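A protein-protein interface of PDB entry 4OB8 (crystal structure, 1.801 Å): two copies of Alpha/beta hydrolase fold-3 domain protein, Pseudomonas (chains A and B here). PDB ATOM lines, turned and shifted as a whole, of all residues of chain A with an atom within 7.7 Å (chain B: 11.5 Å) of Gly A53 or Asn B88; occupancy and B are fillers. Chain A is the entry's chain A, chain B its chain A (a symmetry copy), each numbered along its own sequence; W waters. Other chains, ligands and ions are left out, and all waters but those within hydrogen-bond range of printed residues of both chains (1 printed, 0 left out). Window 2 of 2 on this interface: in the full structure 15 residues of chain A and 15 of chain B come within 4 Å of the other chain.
The backbone carbonyl oxygen (O) of Gly A53 sits at hydrogen-bond distance from the side-chain amide nitrogen (ND2) of Asn B88, at 3.2 Å. O of Ala A56 sits at hydrogen-bond distance from N of Gly B64 (2.7 Å).
The guanidinium group (NE) of Arg B117 sits at hydrogen-bond distance from the backbone carbonyl oxygen (O) of Ser B63. The side-chain carboxylate (OD1) of Asp B61 sits at hydrogen-bond distance from the side-chain hydroxyl (OG) of Ser B63, at 2.7 Å. The side-chain hydroxyl of Thr A52 is in hydrogen-bond range of the backbone carbonyl oxygen of Arg A48, 3.1 Å away. O of Arg B85 lies within hydrogen-bond range of N of Glu B66 (2.8 Å). The backbone NH of Ala B87 sits at hydrogen-bond distance from the backbone carbonyl oxygen of Gly B64.
Thr A52 touches Glu B66 (CG2 to CB, 3.7 Å). Ser B63 touches Ala A56 (CB to O, 3.4 Å). Ala A56 touches Ile B65. Ala A56 touches Ala B87. Val A58 touches Ser B63.
Gly A53 touches one residue of chain B. Printed residues of chain A within 4 Å of Asn B88: Gly A53. No residue of chain B comes within 4 Å of Ala A54. Ala A56 touches just these residues of chain B: Ser B63, Gly B64, Ile B65 and Ala B87. Of chain A, only Ala A56 comes within 4 Å of Ala B87. Of the printed residues of chain A, Gly B64 touches Ala A56 (2.7 Å). Of the printed residues of chain A, Ser B63 touches Ala A56 (3.4 Å) and Val A58 (3.4 Å). Of the printed residues of chain B, Val A58 touches Ser B63. Printed residues of chain A within 4 Å of Ile B65: Ala A56. The nearest residue of chain B that does not touch Gly A53 is Ala B87 (5.0 Å). The nearest printed residue of chain A that does not touch Glu B66 is Ala A56 (5.2 Å).
Of the 24 printed residues of chain B, 6 touch a printed residue of chain A. Hydrophobic or aromatic side chains of chain B within 4 Å of the printed part of chain A: Ala B87. Of the 13 printed residues of chain A, 4 touch a printed residue of chain B. Hydrophobic or aromatic side chains of chain A within 4 Å of the printed part of chain B: Ala A56. Along chain A the printed residues that touch a printed residue of chain B span positions 52 to 58.
No position is printed for both chains. Of the 7 pairs that touch across the chains among the printed residues, none has its exchanged pair printed and touching as well.
Water W1 lies within hydrogen-bond range of OD1 of Asn B88 (2.8 Å), N of Ala A54 (3.4 Å) and O of Gly A53 (3.5 Å).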
ATOM      1  N   ALA A  47      31.926   7.871  -4.999  1.00  0.00           N
ATOM      2  CA  ALA A  47      32.562   8.789  -4.052  1.00  0.00           C
ATOM      3  C   ALA A  47      31.848  10.139  -4.063  1.00  0.00           C
ATOM      4  O   ALA A  47      31.612  10.738  -3.013  1.00  0.00           O
ATOM      5  CB  ALA A  47      34.046   8.964  -4.385  1.00  0.00           C
ATOM      6  N   ARG A  48      31.498  10.611  -5.253  1.00  0.00           N
ATOM      7  CA  ARG A  48      30.769  11.874  -5.389  1.00  0.00           C
ATOM      8  C   ARG A  48      29.432  11.813  -4.662  1.00  0.00           C
ATOM      9  O   ARG A  48      29.017  12.777  -4.016  1.00  0.00           O
ATOM     10  CB  ARG A  48      30.563  12.215  -6.872  1.00  0.00           C
ATOM     11  CG  ARG A  48      31.830  12.724  -7.543  1.00  0.00           C
ATOM     12  CD  ARG A  48      31.840  12.498  -9.056  1.00  0.00           C
ATOM     13  NE  ARG A  48      33.183  12.761  -9.571  1.00  0.00           N
ATOM     14  CZ  ARG A  48      33.614  12.444 -10.786  1.00  0.00           C
ATOM     15  NH1 ARG A  48      32.803  11.842 -11.651  1.00  0.00           N
ATOM     16  NH2 ARG A  48      34.863  12.729 -11.130  1.00  0.00           N
ATOM     17  N   ALA A  49      28.767  10.665  -4.753  1.00  0.00           N
ATOM     18  CA  ALA A  49      27.481  10.475  -4.090  1.00  0.00           C
ATOM     19  C   ALA A  49      27.588  10.521  -2.561  1.00  0.00           C
ATOM     20  O   ALA A  49      26.622  10.870  -1.887  1.00  0.00           O
ATOM     21  CB  ALA A  49      26.845   9.168  -4.540  1.00  0.00           C
ATOM     22  N   VAL A  50      28.744  10.150  -2.011  1.00  0.00           N
ATOM     23  CA  VAL A  50      28.918  10.184  -0.557  1.00  0.00           C
ATOM     24  C   VAL A  50      28.785  11.617  -0.045  1.00  0.00           C
ATOM     25  O   VAL A  50      28.062  11.879   0.922  1.00  0.00           O
ATOM     26  CB  VAL A  50      30.272   9.593  -0.114  1.00  0.00           C
ATOM     27  CG1 VAL A  50      30.483   9.802   1.377  1.00  0.00           C
ATOM     28  CG2 VAL A  50      30.321   8.110  -0.430  1.00  0.00           C
ATOM     29  N   LEU A  51      29.470  12.540  -0.712  1.00  0.00           N
ATOM     30  CA  LEU A  51      29.430  13.950  -0.326  1.00  0.00           C
ATOM     31  C   LEU A  51      28.063  14.552  -0.625  1.00  0.00           C
ATOM     32  O   LEU A  51      27.520  15.307   0.182  1.00  0.00           O
ATOM     33  CB  LEU A  51      30.541  14.736  -1.040  1.00  0.00           C
ATOM     34  CG  LEU A  51      30.541  16.261  -0.845  1.00  0.00           C
ATOM     35  CD1 LEU A  51      30.787  16.647   0.613  1.00  0.00           C
ATOM     36  CD2 LEU A  51      31.574  16.923  -1.752  1.00  0.00           C
ATOM     37  N   THR A  52      27.505  14.219  -1.784  1.00  0.00           N
ATOM     38  CA  THR A  52      26.178  14.721  -2.148  1.00  0.00           C
ATOM     39  C   THR A  52      25.151  14.336  -1.084  1.00  0.00           C
ATOM     40  O   THR A  52      24.397  15.188  -0.583  1.00  0.00           O
ATOM     41  CB  THR A  52      25.746  14.179  -3.520  1.00  0.00           C
ATOM     42  OG1 THR A  52      26.610  14.714  -4.526  1.00  0.00           O
ATOM     43  CG2 THR A  52      24.310  14.570  -3.827  1.00  0.00           C
ATOM     44  N   GLY A  53      25.136  13.053  -0.727  1.00  0.00           N
ATOM     45  CA  GLY A  53      24.170  12.549   0.234  1.00  0.00           C
ATOM     46  C   GLY A  53      24.353  13.113   1.627  1.00  0.00           C
ATOM     47  O   GLY A  53      23.380  13.449   2.306  1.00  0.00           O
ATOM     48  N   ALA A  54      25.606  13.215   2.062  1.00  0.00           N
ATOM     49  CA  ALA A  54      25.888  13.737   3.394  1.00  0.00           C
ATOM     50  C   ALA A  54      25.513  15.216   3.509  1.00  0.00           C
ATOM     51  O   ALA A  54      24.972  15.652   4.535  1.00  0.00           O
ATOM     52  CB  ALA A  54      27.364  13.515   3.755  1.00  0.00           C
ATOM     53  N   GLN A  55      25.807  15.992   2.470  1.00  0.00           N
ATOM     54  CA  GLN A  55      25.487  17.421   2.501  1.00  0.00           C
ATOM     55  C   GLN A  55      23.977  17.648   2.504  1.00  0.00           C
ATOM     56  O   GLN A  55      23.481  18.609   3.090  1.00  0.00           O
ATOM     57  CB  GLN A  55      26.145  18.162   1.325  1.00  0.00           C
ATOM     58  CG  GLN A  55      27.674  18.227   1.395  1.00  0.00           C
ATOM     59  CD  GLN A  55      28.162  19.027   2.594  1.00  0.00           C
ATOM     60  OE1 GLN A  55      28.140  18.544   3.725  1.00  0.00           O
ATOM     61  NE2 GLN A  55      28.588  20.264   2.350  1.00  0.00           N
ATOM     62  N   ALA A  56      23.248  16.745   1.861  1.00  0.00           N
ATOM     63  CA  ALA A  56      21.799  16.879   1.734  1.00  0.00           C
ATOM     64  C   ALA A  56      21.043  16.400   2.976  1.00  0.00           C
ATOM     65  O   ALA A  56      19.830  16.597   3.089  1.00  0.00           O
ATOM     66  CB  ALA A  56      21.321  16.122   0.502  1.00  0.00           C
ATOM     67  N   SER A  57      21.750  15.783   3.916  1.00  0.00           N
ATOM     68  CA  SER A  57      21.079  15.138   5.043  1.00  0.00           C
ATOM     69  C   SER A  57      20.851  16.079   6.216  1.00  0.00           C
ATOM     70  O   SER A  57      20.319  15.669   7.249  1.00  0.00           O
ATOM     71  CB  SER A  57      21.888  13.932   5.510  1.00  0.00           C
ATOM     72  OG  SER A  57      23.073  14.353   6.170  1.00  0.00           O
ATOM     73  N   VAL A  58      21.231  17.344   6.037  1.00  0.00           N
ATOM     74  CA  VAL A  58      21.269  18.310   7.121  1.00  0.00           C
ATOM     75  C   VAL A  58      20.472  19.546   6.739  1.00  0.00           C
ATOM     76  O   VAL A  58      20.718  20.137   5.693  1.00  0.00           O
ATOM     77  CB  VAL A  58      22.727  18.789   7.344  1.00  0.00           C
ATOM     78  CG1 VAL A  58      22.820  19.605   8.592  1.00  0.00           C
ATOM     79  CG2 VAL A  58      23.672  17.610   7.419  1.00  0.00           C
ATOM     80  N   THR A 111      26.961  20.796  -3.421  1.00  0.00           N
ATOM     81  CA  THR A 111      27.628  20.295  -2.217  1.00  0.00           C
ATOM     82  C   THR A 111      28.280  21.434  -1.449  1.00  0.00           C
ATOM     83  O   THR A 111      28.418  21.375  -0.228  1.00  0.00           O
ATOM     84  CB  THR A 111      28.694  19.219  -2.521  1.00  0.00           C
ATOM     85  OG1 THR A 111      29.642  19.713  -3.478  1.00  0.00           O
ATOM     86  CG2 THR A 111      28.039  17.931  -3.055  1.00  0.00           C
ATOM     87  N   ASP B  61      14.034  25.237   4.956  1.00  0.00           N
ATOM     88  CA  ASP B  61      14.660  23.915   4.877  1.00  0.00           C
ATOM     89  C   ASP B  61      14.662  23.422   3.432  1.00  0.00           C
ATOM     90  O   ASP B  61      13.596  23.214   2.853  1.00  0.00           O
ATOM     91  CB  ASP B  61      13.878  22.935   5.757  1.00  0.00           C
ATOM     92  CG  ASP B  61      14.575  21.593   5.934  1.00  0.00           C
ATOM     93  OD1 ASP B  61      15.591  21.330   5.266  1.00  0.00           O
ATOM     94  OD2 ASP B  61      14.085  20.784   6.754  1.00  0.00           O
ATOM     95  N   LEU B  62      15.848  23.245   2.850  1.00  0.00           N
ATOM     96  CA  LEU B  62      15.970  22.700   1.491  1.00  0.00           C
ATOM     97  C   LEU B  62      16.676  21.348   1.476  1.00  0.00           C
ATOM     98  O   LEU B  62      17.107  20.885   0.420  1.00  0.00           O
ATOM     99  CB  LEU B  62      16.721  23.677   0.570  1.00  0.00           C
ATOM    100  CG  LEU B  62      16.053  25.033   0.330  1.00  0.00           C
ATOM    101  CD1 LEU B  62      16.904  25.930  -0.551  1.00  0.00           C
ATOM    102  CD2 LEU B  62      14.683  24.831  -0.301  1.00  0.00           C
ATOM    103  N   SER B  63      16.786  20.712   2.640  1.00  0.00           N
ATOM    104  CA  SER B  63      17.523  19.449   2.763  1.00  0.00           C
ATOM    105  C   SER B  63      16.780  18.274   2.135  1.00  0.00           C
ATOM    106  O   SER B  63      15.594  18.368   1.821  1.00  0.00           O
ATOM    107  CB  SER B  63      17.805  19.137   4.235  1.00  0.00           C
ATOM    108  OG  SER B  63      16.604  18.861   4.938  1.00  0.00           O
ATOM    109  N   GLY B  64      17.488  17.164   1.940  1.00  0.00           N
ATOM    110  CA  GLY B  64      16.843  15.929   1.523  1.00  0.00           C
ATOM    111  C   GLY B  64      16.674  15.785   0.025  1.00  0.00           C
ATOM    112  O   GLY B  64      15.982  14.874  -0.441  1.00  0.00           O
ATOM    113  N   ILE B  65      17.295  16.682  -0.737  1.00  0.00           N
ATOM    114  CA  ILE B  65      17.226  16.612  -2.189  1.00  0.00           C
ATOM    115  C   ILE B  65      18.610  16.728  -2.800  1.00  0.00           C
ATOM    116  O   ILE B  65      19.531  17.283  -2.189  1.00  0.00           O
ATOM    117  CB  ILE B  65      16.339  17.730  -2.777  1.00  0.00           C
ATOM    118  CG1 ILE B  65      16.851  19.113  -2.337  1.00  0.00           C
ATOM    119  CG2 ILE B  65      14.894  17.544  -2.353  1.00  0.00           C
ATOM    120  CD1 ILE B  65      16.194  20.297  -3.079  1.00  0.00           C
ATOM    121  N   GLU B  66      18.756  16.202  -4.009  1.00  0.00           N
ATOM    122  CA  GLU B  66      19.945  16.476  -4.804  1.00  0.00           C
ATOM    123  C   GLU B  66      19.504  17.045  -6.143  1.00  0.00           C
ATOM    124  O   GLU B  66      18.633  16.479  -6.819  1.00  0.00           O
ATOM    125  CB  GLU B  66      20.843  15.243  -4.956  1.00  0.00           C
ATOM    126  CG  GLU B  66      20.237  14.033  -5.629  1.00  0.00           C
ATOM    127  CD  GLU B  66      21.242  12.889  -5.765  1.00  0.00           C
ATOM    128  OE1 GLU B  66      21.291  12.029  -4.864  1.00  0.00           O
ATOM    129  OE2 GLU B  66      21.984  12.862  -6.772  1.00  0.00           O
ATOM    130  N   VAL B  67      20.083  18.190  -6.501  1.00  0.00           N
ATOM    131  CA  VAL B  67      19.646  18.940  -7.673  1.00  0.00           C
ATOM    132  C   VAL B  67      20.703  18.852  -8.759  1.00  0.00           C
ATOM    133  O   VAL B  67      21.881  19.102  -8.501  1.00  0.00           O
ATOM    134  CB  VAL B  67      19.432  20.423  -7.320  1.00  0.00           C
ATOM    135  CG1 VAL B  67      18.971  21.206  -8.539  1.00  0.00           C
ATOM    136  CG2 VAL B  67      18.424  20.559  -6.196  1.00  0.00           C
ATOM    137  N   VAL B  84      15.365  17.182  -9.626  1.00  0.00           N
ATOM    138  CA  VAL B  84      15.431  17.266  -8.168  1.00  0.00           C
ATOM    139  C   VAL B  84      15.054  15.911  -7.596  1.00  0.00           C
ATOM    140  O   VAL B  84      13.889  15.511  -7.632  1.00  0.00           O
ATOM    141  CB  VAL B  84      14.483  18.360  -7.620  1.00  0.00           C
ATOM    142  CG1 VAL B  84      14.650  18.506  -6.108  1.00  0.00           C
ATOM    143  CG2 VAL B  84      14.756  19.695  -8.306  1.00  0.00           C
ATOM    144  N   ARG B  85      16.049  15.205  -7.072  1.00  0.00           N
ATOM    145  CA  ARG B  85      15.885  13.820  -6.655  1.00  0.00           C
ATOM    146  C   ARG B  85      15.918  13.710  -5.134  1.00  0.00           C
ATOM    147  O   ARG B  85      16.675  14.429  -4.479  1.00  0.00           O
ATOM    148  CB  ARG B  85      17.029  13.001  -7.261  1.00  0.00           C
ATOM    149  CG  ARG B  85      16.983  11.513  -6.981  1.00  0.00           C
ATOM    150  CD  ARG B  85      18.283  10.835  -7.431  1.00  0.00           C
ATOM    151  NE  ARG B  85      18.247   9.408  -7.105  1.00  0.00           N
ATOM    152  CZ  ARG B  85      17.694   8.485  -7.885  1.00  0.00           C
ATOM    153  NH1 ARG B  85      17.153   8.836  -9.044  1.00  0.00           N
ATOM    154  NH2 ARG B  85      17.686   7.208  -7.512  1.00  0.00           N
ATOM    155  N   PRO B  86      15.097  12.813  -4.559  1.00  0.00           N
ATOM    156  CA  PRO B  86      15.263  12.537  -3.126  1.00  0.00           C
ATOM    157  C   PRO B  86      16.690  12.070  -2.849  1.00  0.00           C
ATOM    158  O   PRO B  86      17.218  11.226  -3.578  1.00  0.00           O
ATOM    159  CB  PRO B  86      14.278  11.396  -2.868  1.00  0.00           C
ATOM    160  CG  PRO B  86      13.210  11.573  -3.923  1.00  0.00           C
ATOM    161  CD  PRO B  86      13.954  12.088  -5.144  1.00  0.00           C
ATOM    162  N   ALA B  87      17.316  12.629  -1.819  1.00  0.00           N
ATOM    163  CA  ALA B  87      18.712  12.316  -1.524  1.00  0.00           C
ATOM    164  C   ALA B  87      18.868  10.913  -0.947  1.00  0.00           C
ATOM    165  O   ALA B  87      17.957  10.395  -0.295  1.00  0.00           O
ATOM    166  CB  ALA B  87      19.295  13.355  -0.561  1.00  0.00           C
ATOM    167  N   ASN B  88      20.035  10.320  -1.175  1.00  0.00           N
ATOM    168  CA  ASN B  88      20.389   9.024  -0.594  1.00  0.00           C
ATOM    169  C   ASN B  88      19.439   7.893  -0.974  1.00  0.00           C
ATOM    170  O   ASN B  88      19.161   7.017  -0.160  1.00  0.00           O
ATOM    171  CB  ASN B  88      20.493   9.131   0.932  1.00  0.00           C
ATOM    172  CG  ASN B  88      21.559  10.113   1.371  1.00  0.00           C
ATOM    173  OD1 ASN B  88      22.748   9.889   1.140  1.00  0.00           O
ATOM    174  ND2 ASN B  88      21.141  11.206   2.007  1.00  0.00           N
ATOM    175  N   VAL B  89      18.939   7.917  -2.204  1.00  0.00           N
ATOM    176  CA  VAL B  89      18.049   6.862  -2.674  1.00  0.00           C
ATOM    177  C   VAL B  89      18.621   6.288  -3.956  1.00  0.00           C
ATOM    178  O   VAL B  89      18.982   7.032  -4.864  1.00  0.00           O
ATOM    179  CB  VAL B  89      16.611   7.377  -2.930  1.00  0.00           C
ATOM    180  CG1 VAL B  89      15.735   6.255  -3.470  1.00  0.00           C
ATOM    181  CG2 VAL B  89      16.009   7.943  -1.654  1.00  0.00           C
ATOM    182  N   LYS B  90      18.715   4.963  -4.023  1.00  0.00           N
ATOM    183  CA  LYS B  90      19.263   4.302  -5.198  1.00  0.00           C
ATOM    184  C   LYS B  90      18.159   3.775  -6.100  1.00  0.00           C
ATOM    185  O   LYS B  90      17.064   3.453  -5.629  1.00  0.00           O
ATOM    186  CB  LYS B  90      20.176   3.148  -4.780  1.00  0.00           C
ATOM    187  CG  LYS B  90      21.465   3.593  -4.110  1.00  0.00           C
ATOM    188  CD  LYS B  90      22.023   2.489  -3.225  1.00  0.00           C
ATOM    189  CE  LYS B  90      23.389   2.858  -2.668  1.00  0.00           C
ATOM    190  NZ  LYS B  90      23.350   4.102  -1.847  1.00  0.00           N
ATOM    191  N   GLY B  91      18.449   3.708  -7.395  1.00  0.00           N
ATOM    192  CA  GLY B  91      17.556   3.087  -8.353  1.00  0.00           C
ATOM    193  C   GLY B  91      16.638   4.036  -9.095  1.00  0.00           C
ATOM    194  O   GLY B  91      16.608   5.246  -8.830  1.00  0.00           O
ATOM    195  N   GLU B  92      15.886   3.480 -10.038  1.00  0.00           N
ATOM    196  CA  GLU B  92      14.905   4.254 -10.780  1.00  0.00           C
ATOM    197  C   GLU B  92      13.804   4.707  -9.831  1.00  0.00           C
ATOM    198  O   GLU B  92      13.367   3.947  -8.962  1.00  0.00           O
ATOM    199  CB  GLU B  92      14.288   3.416 -11.898  1.00  0.00           C
ATOM    200  CG  GLU B  92      15.039   3.441 -13.207  1.00  0.00           C
ATOM    201  CD  GLU B  92      14.238   2.797 -14.330  1.00  0.00           C
ATOM    202  OE1 GLU B  92      13.090   2.357 -14.076  1.00  0.00           O
ATOM    203  OE2 GLU B  92      14.757   2.740 -15.461  1.00  0.00           O
ATOM    204  N   LEU B  93      13.365   5.950  -9.992  1.00  0.00           N
ATOM    205  CA  LEU B  93      12.268   6.478  -9.196  1.00  0.00           C
ATOM    206  C   LEU B  93      11.200   6.999 -10.137  1.00  0.00           C
ATOM    207  O   LEU B  93      11.502   7.385 -11.273  1.00  0.00           O
ATOM    208  CB  LEU B  93      12.763   7.626  -8.307  1.00  0.00           C
ATOM    209  CG  LEU B  93      13.655   7.228  -7.132  1.00  0.00           C
ATOM    210  CD1 LEU B  93      14.202   8.464  -6.425  1.00  0.00           C
ATOM    211  CD2 LEU B  93      12.866   6.375  -6.162  1.00  0.00           C
ATOM    212  N   ARG B 117      11.124  21.260  -3.445  1.00  0.00           N
ATOM    213  CA  ARG B 117      11.757  20.409  -2.440  1.00  0.00           C
ATOM    214  C   ARG B 117      10.709  19.747  -1.562  1.00  0.00           C
ATOM    215  O   ARG B 117      10.804  18.554  -1.274  1.00  0.00           O
ATOM    216  CB  ARG B 117      12.734  21.231  -1.584  1.00  0.00           C
ATOM    217  CG  ARG B 117      13.376  20.451  -0.440  1.00  0.00           C
ATOM    218  CD  ARG B 117      12.646  20.674   0.886  1.00  0.00           C
ATOM    219  NE  ARG B 117      13.226  19.860   1.954  1.00  0.00           N
ATOM    220  CZ  ARG B 117      12.595  19.535   3.077  1.00  0.00           C
ATOM    221  NH1 ARG B 117      13.210  18.788   3.984  1.00  0.00           N
ATOM    222  NH2 ARG B 117      11.347  19.936   3.287  1.00  0.00           N
ATOM    223  N   VAL B 120       9.083  16.958  -3.534  1.00  0.00           N
ATOM    224  CA  VAL B 120       9.995  15.829  -3.696  1.00  0.00           C
ATOM    225  C   VAL B 120      10.169  15.039  -2.397  1.00  0.00           C
ATOM    226  O   VAL B 120      10.022  13.808  -2.378  1.00  0.00           O
ATOM    227  CB  VAL B 120      11.362  16.312  -4.200  1.00  0.00           C
ATOM    228  CG1 VAL B 120      12.395  15.198  -4.121  1.00  0.00           C
ATOM    229  CG2 VAL B 120      11.229  16.821  -5.628  1.00  0.00           C
ATOM    230  N   VAL B 121      10.486  15.734  -1.308  1.00  0.00           N
ATOM    231  CA  VAL B 121      10.735  15.038  -0.046  1.00  0.00           C
ATOM    232  C   VAL B 121       9.473  14.328   0.437  1.00  0.00           C
ATOM    233  O   VAL B 121       9.534  13.208   0.957  1.00  0.00           O
ATOM    234  CB  VAL B 121      11.282  15.996   1.036  1.00  0.00           C
ATOM    235  CG1 VAL B 121      11.318  15.320   2.394  1.00  0.00           C
ATOM    236  CG2 VAL B 121      12.675  16.461   0.644  1.00  0.00           C
ATOM    237  N   GLY B 124       8.762  11.292  -2.371  1.00  0.00           N
ATOM    238  CA  GLY B 124       9.794  10.318  -2.698  1.00  0.00           C
ATOM    239  C   GLY B 124       9.999  10.171  -4.193  1.00  0.00           C
ATOM    240  O   GLY B 124      10.719   9.279  -4.649  1.00  0.00           O
ATOM    241  N   ALA B 125       9.366  11.051  -4.963  1.00  0.00           N
ATOM    242  CA  ALA B 125       9.485  11.037  -6.417  1.00  0.00           C
ATOM    243  C   ALA B 125      10.403  12.151  -6.893  1.00  0.00           C
ATOM    244  O   ALA B 125      10.610  13.141  -6.195  1.00  0.00           O
ATOM    245  CB  ALA B 125       8.114  11.190  -7.075  1.00  0.00           C
ATOM    246  N   VAL B 126      10.923  12.002  -8.104  1.00  0.00           N
ATOM    247  CA  VAL B 126      11.826  12.994  -8.674  1.00  0.00           C
ATOM    248  C   VAL B 126      11.018  14.090  -9.357  1.00  0.00           C
ATOM    249  O   VAL B 126      10.066  13.785 -10.066  1.00  0.00           O
ATOM    250  CB  VAL B 126      12.752  12.336  -9.710  1.00  0.00           C
ATOM    251  CG1 VAL B 126      13.527  13.388 -10.494  1.00  0.00           C
ATOM    252  CG2 VAL B 126      13.709  11.351  -9.021  1.00  0.00           C
ATOM    253  N   GLY B 162      17.700   8.919 -14.338  1.00  0.00           N
ATOM    254  CA  GLY B 162      17.456   8.112 -13.152  1.00  0.00           C
ATOM    255  C   GLY B 162      15.997   7.946 -12.768  1.00  0.00           C
ATOM    256  O   GLY B 162      15.685   7.679 -11.604  1.00  0.00           O
HETATM  257  O   HOH W   1      24.467  10.304   3.355  1.00  0.00           O
